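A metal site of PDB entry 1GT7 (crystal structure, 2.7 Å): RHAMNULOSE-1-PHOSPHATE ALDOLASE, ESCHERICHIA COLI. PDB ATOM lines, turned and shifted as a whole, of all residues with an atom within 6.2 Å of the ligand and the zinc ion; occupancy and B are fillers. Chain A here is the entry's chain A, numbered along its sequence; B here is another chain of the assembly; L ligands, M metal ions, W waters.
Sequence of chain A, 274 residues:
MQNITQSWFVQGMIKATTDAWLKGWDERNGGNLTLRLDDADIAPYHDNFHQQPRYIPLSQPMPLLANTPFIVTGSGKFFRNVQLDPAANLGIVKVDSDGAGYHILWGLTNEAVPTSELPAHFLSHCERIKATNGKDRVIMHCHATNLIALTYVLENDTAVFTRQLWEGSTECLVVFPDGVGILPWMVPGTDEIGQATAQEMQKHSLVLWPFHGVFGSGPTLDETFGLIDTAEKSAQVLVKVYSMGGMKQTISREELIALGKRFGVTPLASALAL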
ATOM      1  N   ASN A  29     -14.912  14.950  -0.244  1.00  0.00           N
ATOM      2  CA  ASN A  29     -13.900  14.418  -1.158  1.00  0.00           C
ATOM      3  C   ASN A  29     -13.632  15.367  -2.331  1.00  0.00           C
ATOM      4  O   ASN A  29     -12.958  15.010  -3.337  1.00  0.00           O
ATOM      5  CB  ASN A  29     -14.380  13.083  -1.669  1.00  0.00           C
ATOM      6  CG  ASN A  29     -15.643  13.241  -2.517  1.00  0.00           C
ATOM      7  OD1 ASN A  29     -16.699  13.734  -2.066  1.00  0.00           O
ATOM      8  ND2 ASN A  29     -15.505  12.806  -3.766  1.00  0.00           N
ATOM      9  N   GLY A  30     -14.125  16.608  -2.199  1.00  0.00           N
ATOM     10  CA  GLY A  30     -13.924  17.607  -3.203  1.00  0.00           C
ATOM     11  C   GLY A  30     -12.481  17.872  -3.512  1.00  0.00           C
ATOM     12  O   GLY A  30     -11.610  18.056  -2.664  1.00  0.00           O
ATOM     13  N   GLY A  31     -12.166  17.879  -4.793  1.00  0.00           N
ATOM     14  CA  GLY A  31     -10.821  18.094  -5.328  1.00  0.00           C
ATOM     15  C   GLY A  31     -10.110  16.781  -5.569  1.00  0.00           C
ATOM     16  O   GLY A  31     -10.576  15.680  -5.175  1.00  0.00           O
ATOM     17  N   ASN A  32      -9.015  16.886  -6.302  1.00  0.00           N
ATOM     18  CA  ASN A  32      -8.173  15.756  -6.626  1.00  0.00           C
ATOM     19  C   ASN A  32      -6.859  16.338  -7.154  1.00  0.00           C
ATOM     20  O   ASN A  32      -6.815  17.441  -7.647  1.00  0.00           O
ATOM     21  CB  ASN A  32      -8.818  14.755  -7.545  1.00  0.00           C
ATOM     22  CG  ASN A  32      -9.823  15.413  -8.452  1.00  0.00           C
ATOM     23  OD1 ASN A  32      -9.539  16.228  -9.330  1.00  0.00           O
ATOM     24  ND2 ASN A  32     -11.061  15.093  -8.212  1.00  0.00           N
ATOM     25  N   THR A  73      -4.529  11.303  -5.829  1.00  0.00           N
ATOM     26  CA  THR A  73      -5.454  11.203  -4.683  1.00  0.00           C
ATOM     27  C   THR A  73      -6.502  10.172  -5.028  1.00  0.00           C
ATOM     28  O   THR A  73      -6.657   9.878  -6.189  1.00  0.00           O
ATOM     29  CB  THR A  73      -6.064  12.532  -4.348  1.00  0.00           C
ATOM     30  OG1 THR A  73      -6.642  13.087  -5.523  1.00  0.00           O
ATOM     31  CG2 THR A  73      -5.052  13.516  -3.882  1.00  0.00           C
ATOM     32  N   GLY A  74      -7.161   9.498  -4.130  1.00  0.00           N
ATOM     33  CA  GLY A  74      -8.120   8.459  -4.386  1.00  0.00           C
ATOM     34  C   GLY A  74      -9.510   8.963  -4.551  1.00  0.00           C
ATOM     35  O   GLY A  74      -9.926  10.045  -4.074  1.00  0.00           O
ATOM     36  N   SER A  75     -10.303   8.140  -5.228  1.00  0.00           N
ATOM     37  CA  SER A  75     -11.727   8.433  -5.434  1.00  0.00           C
ATOM     38  C   SER A  75     -12.501   8.417  -4.133  1.00  0.00           C
ATOM     39  O   SER A  75     -12.402   7.459  -3.406  1.00  0.00           O
ATOM     40  CB  SER A  75     -12.352   7.439  -6.400  1.00  0.00           C
ATOM     41  OG  SER A  75     -13.715   7.793  -6.618  1.00  0.00           O
ATOM     42  N   GLY A  76     -13.230   9.446  -3.772  1.00  0.00           N
ATOM     43  CA  GLY A  76     -13.989   9.486  -2.548  1.00  0.00           C
ATOM     44  C   GLY A  76     -13.159   9.798  -1.331  1.00  0.00           C
ATOM     45  O   GLY A  76     -13.697   9.864  -0.225  1.00  0.00           O
ATOM     46  N   LYS A  77     -11.876   9.978  -1.445  1.00  0.00           N
ATOM     47  CA  LYS A  77     -10.999  10.275  -0.322  1.00  0.00           C
ATOM     48  C   LYS A  77     -10.985  11.748   0.022  1.00  0.00           C
ATOM     49  O   LYS A  77     -11.107  12.624  -0.846  1.00  0.00           O
ATOM     50  CB  LYS A  77      -9.601   9.772  -0.708  1.00  0.00           C
ATOM     51  CG  LYS A  77      -9.501   8.290  -1.030  1.00  0.00           C
ATOM     52  CD  LYS A  77     -10.270   7.476  -0.035  1.00  0.00           C
ATOM     53  CE  LYS A  77     -10.113   6.007  -0.327  1.00  0.00           C
ATOM     54  NZ  LYS A  77     -10.918   5.127   0.566  1.00  0.00           N
ATOM     55  N   PRO A 114      -7.901   5.350  -8.044  1.00  0.00           N
ATOM     56  CA  PRO A 114      -7.549   6.750  -8.278  1.00  0.00           C
ATOM     57  C   PRO A 114      -8.799   7.626  -8.401  1.00  0.00           C
ATOM     58  O   PRO A 114      -9.899   7.168  -8.655  1.00  0.00           O
ATOM     59  CB  PRO A 114      -6.800   6.686  -9.601  1.00  0.00           C
ATOM     60  CG  PRO A 114      -6.276   5.321  -9.608  1.00  0.00           C
ATOM     61  CD  PRO A 114      -7.372   4.473  -9.067  1.00  0.00           C
ATOM     62  N   THR A 115      -8.643   8.935  -8.272  1.00  0.00           N
ATOM     63  CA  THR A 115      -9.747   9.869  -8.418  1.00  0.00           C
ATOM     64  C   THR A 115     -10.613   9.598  -9.618  1.00  0.00           C
ATOM     65  O   THR A 115     -10.136   9.315 -10.706  1.00  0.00           O
ATOM     66  CB  THR A 115      -9.197  11.310  -8.580  1.00  0.00           C
ATOM     67  OG1 THR A 115     -10.294  12.192  -8.975  1.00  0.00           O
ATOM     68  CG2 THR A 115      -8.133  11.388  -9.625  1.00  0.00           C
ATOM     69  N   SER A 116     -11.898   9.764  -9.480  1.00  0.00           N
ATOM     70  CA  SER A 116     -12.831   9.610 -10.597  1.00  0.00           C
ATOM     71  C   SER A 116     -12.608  10.704 -11.646  1.00  0.00           C
ATOM     72  O   SER A 116     -13.216  10.652 -12.678  1.00  0.00           O
ATOM     73  CB  SER A 116     -14.279   9.625 -10.082  1.00  0.00           C
ATOM     74  OG  SER A 116     -14.586  10.944  -9.615  1.00  0.00           O
ATOM     75  N   GLU A 117     -11.790  11.727 -11.417  1.00  0.00           N
ATOM     76  CA  GLU A 117     -11.475  12.690 -12.428  1.00  0.00           C
ATOM     77  C   GLU A 117     -10.152  12.346 -13.119  1.00  0.00           C
ATOM     78  O   GLU A 117      -9.526  13.238 -13.674  1.00  0.00           O
ATOM     79  CB  GLU A 117     -11.389  14.113 -11.944  1.00  0.00           C
ATOM     80  CG  GLU A 117     -12.650  14.622 -11.267  1.00  0.00           C
ATOM     81  CD  GLU A 117     -13.817  14.956 -12.192  1.00  0.00           C
ATOM     82  OE1 GLU A 117     -14.808  15.506 -11.631  1.00  0.00           O
ATOM     83  OE2 GLU A 117     -13.784  14.676 -13.406  1.00  0.00           O
ATOM     84  N   HIS A 141      -7.043  20.044  -8.831  1.00  0.00           N
ATOM     85  CA  HIS A 141      -8.425  20.433  -8.934  1.00  0.00           C
ATOM     86  C   HIS A 141      -8.962  20.726  -7.533  1.00  0.00           C
ATOM     87  O   HIS A 141      -8.791  19.853  -6.654  1.00  0.00           O
ATOM     88  CB  HIS A 141      -9.305  19.365  -9.579  1.00  0.00           C
ATOM     89  CG  HIS A 141     -10.772  19.545  -9.387  1.00  0.00           C
ATOM     90  ND1 HIS A 141     -11.512  20.673  -9.773  1.00  0.00           N
ATOM     91  CD2 HIS A 141     -11.720  18.729  -8.835  1.00  0.00           C
ATOM     92  CE1 HIS A 141     -12.760  20.497  -9.447  1.00  0.00           C
ATOM     93  NE2 HIS A 141     -12.963  19.345  -8.898  1.00  0.00           N
ATOM     94  N   CYS A 142      -9.643  21.843  -7.290  1.00  0.00           N
ATOM     95  CA  CYS A 142     -10.244  22.068  -5.991  1.00  0.00           C
ATOM     96  C   CYS A 142     -11.466  22.926  -6.137  1.00  0.00           C
ATOM     97  O   CYS A 142     -11.792  23.485  -7.192  1.00  0.00           O
ATOM     98  CB  CYS A 142      -9.246  22.654  -5.045  1.00  0.00           C
ATOM     99  SG  CYS A 142      -8.729  24.309  -5.453  1.00  0.00           S
ATOM    100  N   HIS A 143     -12.268  23.011  -5.103  1.00  0.00           N
ATOM    101  CA  HIS A 143     -13.535  23.763  -5.087  1.00  0.00           C
ATOM    102  C   HIS A 143     -13.251  25.124  -4.467  1.00  0.00           C
ATOM    103  O   HIS A 143     -13.664  25.418  -3.362  1.00  0.00           O
ATOM    104  CB  HIS A 143     -14.544  22.948  -4.253  1.00  0.00           C
ATOM    105  CG  HIS A 143     -14.857  21.655  -4.976  1.00  0.00           C
ATOM    106  ND1 HIS A 143     -15.692  20.658  -4.475  1.00  0.00           N
ATOM    107  CD2 HIS A 143     -14.408  21.158  -6.140  1.00  0.00           C
ATOM    108  CE1 HIS A 143     -15.768  19.664  -5.330  1.00  0.00           C
ATOM    109  NE2 HIS A 143     -14.996  19.938  -6.365  1.00  0.00           N
ATOM    110  N   PRO A 188     -19.557  16.049 -14.393  1.00  0.00           N
ATOM    111  CA  PRO A 188     -18.216  15.713 -13.962  1.00  0.00           C
ATOM    112  C   PRO A 188     -17.941  14.217 -13.987  1.00  0.00           C
ATOM    113  O   PRO A 188     -18.795  13.361 -13.815  1.00  0.00           O
ATOM    114  CB  PRO A 188     -18.153  16.225 -12.539  1.00  0.00           C
ATOM    115  CG  PRO A 188     -19.531  16.081 -12.028  1.00  0.00           C
ATOM    116  CD  PRO A 188     -20.425  16.433 -13.211  1.00  0.00           C
ATOM    117  N   GLY A 189     -16.644  13.873 -14.007  1.00  0.00           N
ATOM    118  CA  GLY A 189     -16.130  12.528 -13.884  1.00  0.00           C
ATOM    119  C   GLY A 189     -16.240  11.755 -15.180  1.00  0.00           C
ATOM    120  O   GLY A 189     -16.160  10.510 -15.163  1.00  0.00           O
ATOM    121  N   TRP A 209     -14.650  25.298 -14.027  1.00  0.00           N
ATOM    122  CA  TRP A 209     -15.794  24.444 -14.262  1.00  0.00           C
ATOM    123  C   TRP A 209     -16.926  25.144 -13.500  1.00  0.00           C
ATOM    124  O   TRP A 209     -16.876  25.010 -12.276  1.00  0.00           O
ATOM    125  CB  TRP A 209     -15.575  23.094 -13.653  1.00  0.00           C
ATOM    126  CG  TRP A 209     -14.693  22.144 -14.407  1.00  0.00           C
ATOM    127  CD1 TRP A 209     -13.952  22.394 -15.528  1.00  0.00           C
ATOM    128  CD2 TRP A 209     -14.462  20.763 -14.119  1.00  0.00           C
ATOM    129  NE1 TRP A 209     -13.312  21.278 -15.946  1.00  0.00           N
ATOM    130  CE2 TRP A 209     -13.589  20.276 -15.088  1.00  0.00           C
ATOM    131  CE3 TRP A 209     -14.924  19.909 -13.100  1.00  0.00           C
ATOM    132  CZ2 TRP A 209     -13.165  18.943 -15.071  1.00  0.00           C
ATOM    133  CZ3 TRP A 209     -14.488  18.598 -13.103  1.00  0.00           C
ATOM    134  CH2 TRP A 209     -13.638  18.137 -14.094  1.00  0.00           C
ATOM    135  N   HIS A 212     -18.706  24.561  -9.976  1.00  0.00           N
ATOM    136  CA  HIS A 212     -17.965  23.406  -9.579  1.00  0.00           C
ATOM    137  C   HIS A 212     -16.604  23.709  -8.969  1.00  0.00           C
ATOM    138  O   HIS A 212     -16.425  23.519  -7.776  1.00  0.00           O
ATOM    139  CB  HIS A 212     -17.900  22.371 -10.693  1.00  0.00           C
ATOM    140  CG  HIS A 212     -17.299  21.062 -10.252  1.00  0.00           C
ATOM    141  ND1 HIS A 212     -17.526  19.866 -10.832  1.00  0.00           N
ATOM    142  CD2 HIS A 212     -16.416  20.787  -9.301  1.00  0.00           C
ATOM    143  CE1 HIS A 212     -16.846  18.920 -10.302  1.00  0.00           C
ATOM    144  NE2 HIS A 212     -16.163  19.448  -9.319  1.00  0.00           N
ATOM    145  N   GLY A 213     -15.647  24.150  -9.749  1.00  0.00           N
ATOM    146  CA  GLY A 213     -14.343  24.506  -9.255  1.00  0.00           C
ATOM    147  C   GLY A 213     -13.301  24.911 -10.284  1.00  0.00           C
ATOM    148  O   GLY A 213     -13.623  25.381 -11.354  1.00  0.00           O
ATOM    149  N   PHE A 215      -9.199  23.946 -12.121  1.00  0.00           N
ATOM    150  CA  PHE A 215      -8.163  23.031 -12.488  1.00  0.00           C
ATOM    151  C   PHE A 215      -6.918  23.870 -12.818  1.00  0.00           C
ATOM    152  O   PHE A 215      -7.053  24.839 -13.541  1.00  0.00           O
ATOM    153  CB  PHE A 215      -8.431  22.203 -13.736  1.00  0.00           C
ATOM    154  CG  PHE A 215      -9.098  20.928 -13.442  1.00  0.00           C
ATOM    155  CD1 PHE A 215     -10.399  20.906 -13.013  1.00  0.00           C
ATOM    156  CD2 PHE A 215      -8.409  19.747 -13.546  1.00  0.00           C
ATOM    157  CE1 PHE A 215     -11.019  19.684 -12.740  1.00  0.00           C
ATOM    158  CE2 PHE A 215      -8.999  18.525 -13.232  1.00  0.00           C
ATOM    159  CZ  PHE A 215     -10.315  18.489 -12.817  1.00  0.00           C
ATOM    160  N   GLU B 171     -21.555  18.919  -6.700  1.00  0.00           N
ATOM    161  CA  GLU B 171     -21.606  17.631  -6.041  1.00  0.00           C
ATOM    162  C   GLU B 171     -22.842  17.460  -5.169  1.00  0.00           C
ATOM    163  O   GLU B 171     -23.085  16.316  -4.747  1.00  0.00           O
ATOM    164  CB  GLU B 171     -20.345  17.542  -5.160  1.00  0.00           C
ATOM    165  CG  GLU B 171     -20.442  18.531  -4.019  1.00  0.00           C
ATOM    166  CD  GLU B 171     -19.209  19.034  -3.334  1.00  0.00           C
ATOM    167  OE1 GLU B 171     -18.103  18.471  -3.454  1.00  0.00           O
ATOM    168  OE2 GLU B 171     -19.282  20.077  -2.645  1.00  0.00           O
HETATM  169  C1  LIG L   1     -14.259  15.986  -7.341  1.00  0.00           C
HETATM  170  C2  LIG L   1     -14.285  14.786  -6.491  1.00  0.00           C
HETATM  171  N1  LIG L   1     -14.662  15.806  -8.565  1.00  0.00           N
HETATM  172  O1  LIG L   1     -14.779  16.868  -9.440  1.00  0.00           O
HETATM  173  O2  LIG L   1     -13.906  17.030  -6.824  1.00  0.00           O
HETATM  174  O3  LIG L   1     -13.877  13.592  -7.124  1.00  0.00           O
HETATM  175  O4  LIG L   1     -11.381  12.798  -6.892  1.00  0.00           O
HETATM  176  O5  LIG L   1     -12.979  12.362  -4.629  1.00  0.00           O
HETATM  177  O6  LIG L   1     -13.271  11.004  -7.026  1.00  0.00           O
HETATM  178  P1  LIG L   1     -12.820  12.395  -6.270  1.00  0.00           P
HETATM  179 ZN    ZN M   1     -14.794  18.524  -8.104  1.00  0.00          ZN
HETATM  180  O   HOH W   1     -10.514  14.014  -3.261  1.00  0.00           O
HETATM  181  O   HOH W   2     -16.746  17.559  -7.290  1.00  0.00           O
HETATM  182  O   HOH W   3      -9.133  12.428  -5.148  1.00  0.00           O
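Three residues have an atom within 4 Å of the zinc ion: His 141, His 143 and His 212.
The nearest printed residue that does not touch the zinc ion is Gly 31 (4.3 Å).
Water W3 lies within hydrogen-bond range of OG1 of Thr 73 (2.6 Å), O of Gly 74 (2.7 Å) and O4 of the ligand (2.9 Å).
Gly 30 touches the ligand (CA to O2, 3.7 Å).
Gly 74 touches the ligand (O to O5, 3.9 Å).
Hydrophobic or aromatic side chains within 4 Å of the ligand: His 141, His 143 and His 212.
The nearest printed residue that does not touch the ligand is Trp 209 (4.1 Å).
The zinc ion is bound by NE2 of His 212 (2.1 Å), O1 of the ligand (2.1 Å), O2 of the ligand (2.2 Å), NE2 of His 141 (2.2 Å), NE2 of His 143 (2.3 Å) and water W2 (2.3 Å).
The zinc ion has six donor atoms within binding distance.
The side-chain hydroxyl (OG1) of Thr 115 is in hydrogen-bond range of an oxygen (O4) of the ligand (2.4 Å).
The side-chain carboxylate (OE1) of Glu 117 lies within hydrogen-bond range of a nitrogen (N1) of the ligand.
The side-chain amide nitrogen (ND2) of Asn 32 lies within hydrogen-bond range of an oxygen (O4) of the ligand (2.7 Å).
An oxygen (O5) of the ligand sits close to the backbone carbonyl oxygen (O) of Asn 29 (2.9 Å).
The side-chain amide nitrogen of Asn 29 is in hydrogen-bond range of an oxygen (O5) of the ligand, 2.7 Å away.
O2 of the ligand lies close to N of Gly 31, at 2.8 Å.
O6 of the ligand lies within hydrogen-bond range of N of Ser 116, 3.1 Å away.
The side-chain hydroxyl of Ser 116 lies within hydrogen-bond range of an oxygen (O6) of the ligand (2.9 Å).
An oxygen (O5) of the ligand lies within hydrogen-bond range of the backbone NH (N) of Gly 76, at 3.0 Å.
OG of Ser 75 sits at hydrogen-bond distance from O6 of the ligand, at 3.3 Å.
N of His 141 lies within hydrogen-bond range of O of Asn 32.
A ring nitrogen (ND1) of His 143 lies close to the side-chain carboxylate (OE1) of Glu 171 of chain B (3.4 Å).
The backbone NH of Glu 117 lies within hydrogen-bond range of the side-chain hydroxyl of Thr 115, 2.9 Å away.
The side-chain hydroxyl (OG1) of Thr 115 is in hydrogen-bond range of the side-chain amide nitrogen (ND2) of Asn 32, at 3.1 Å.
The backbone carbonyl oxygen (O) of Thr 73 is in hydrogen-bond range of the backbone NH (N) of Thr 115 (3.0 Å).
The side-chain carboxylate of Glu 117 lies within hydrogen-bond range of the backbone NH of Gly 189 (3.0 Å).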
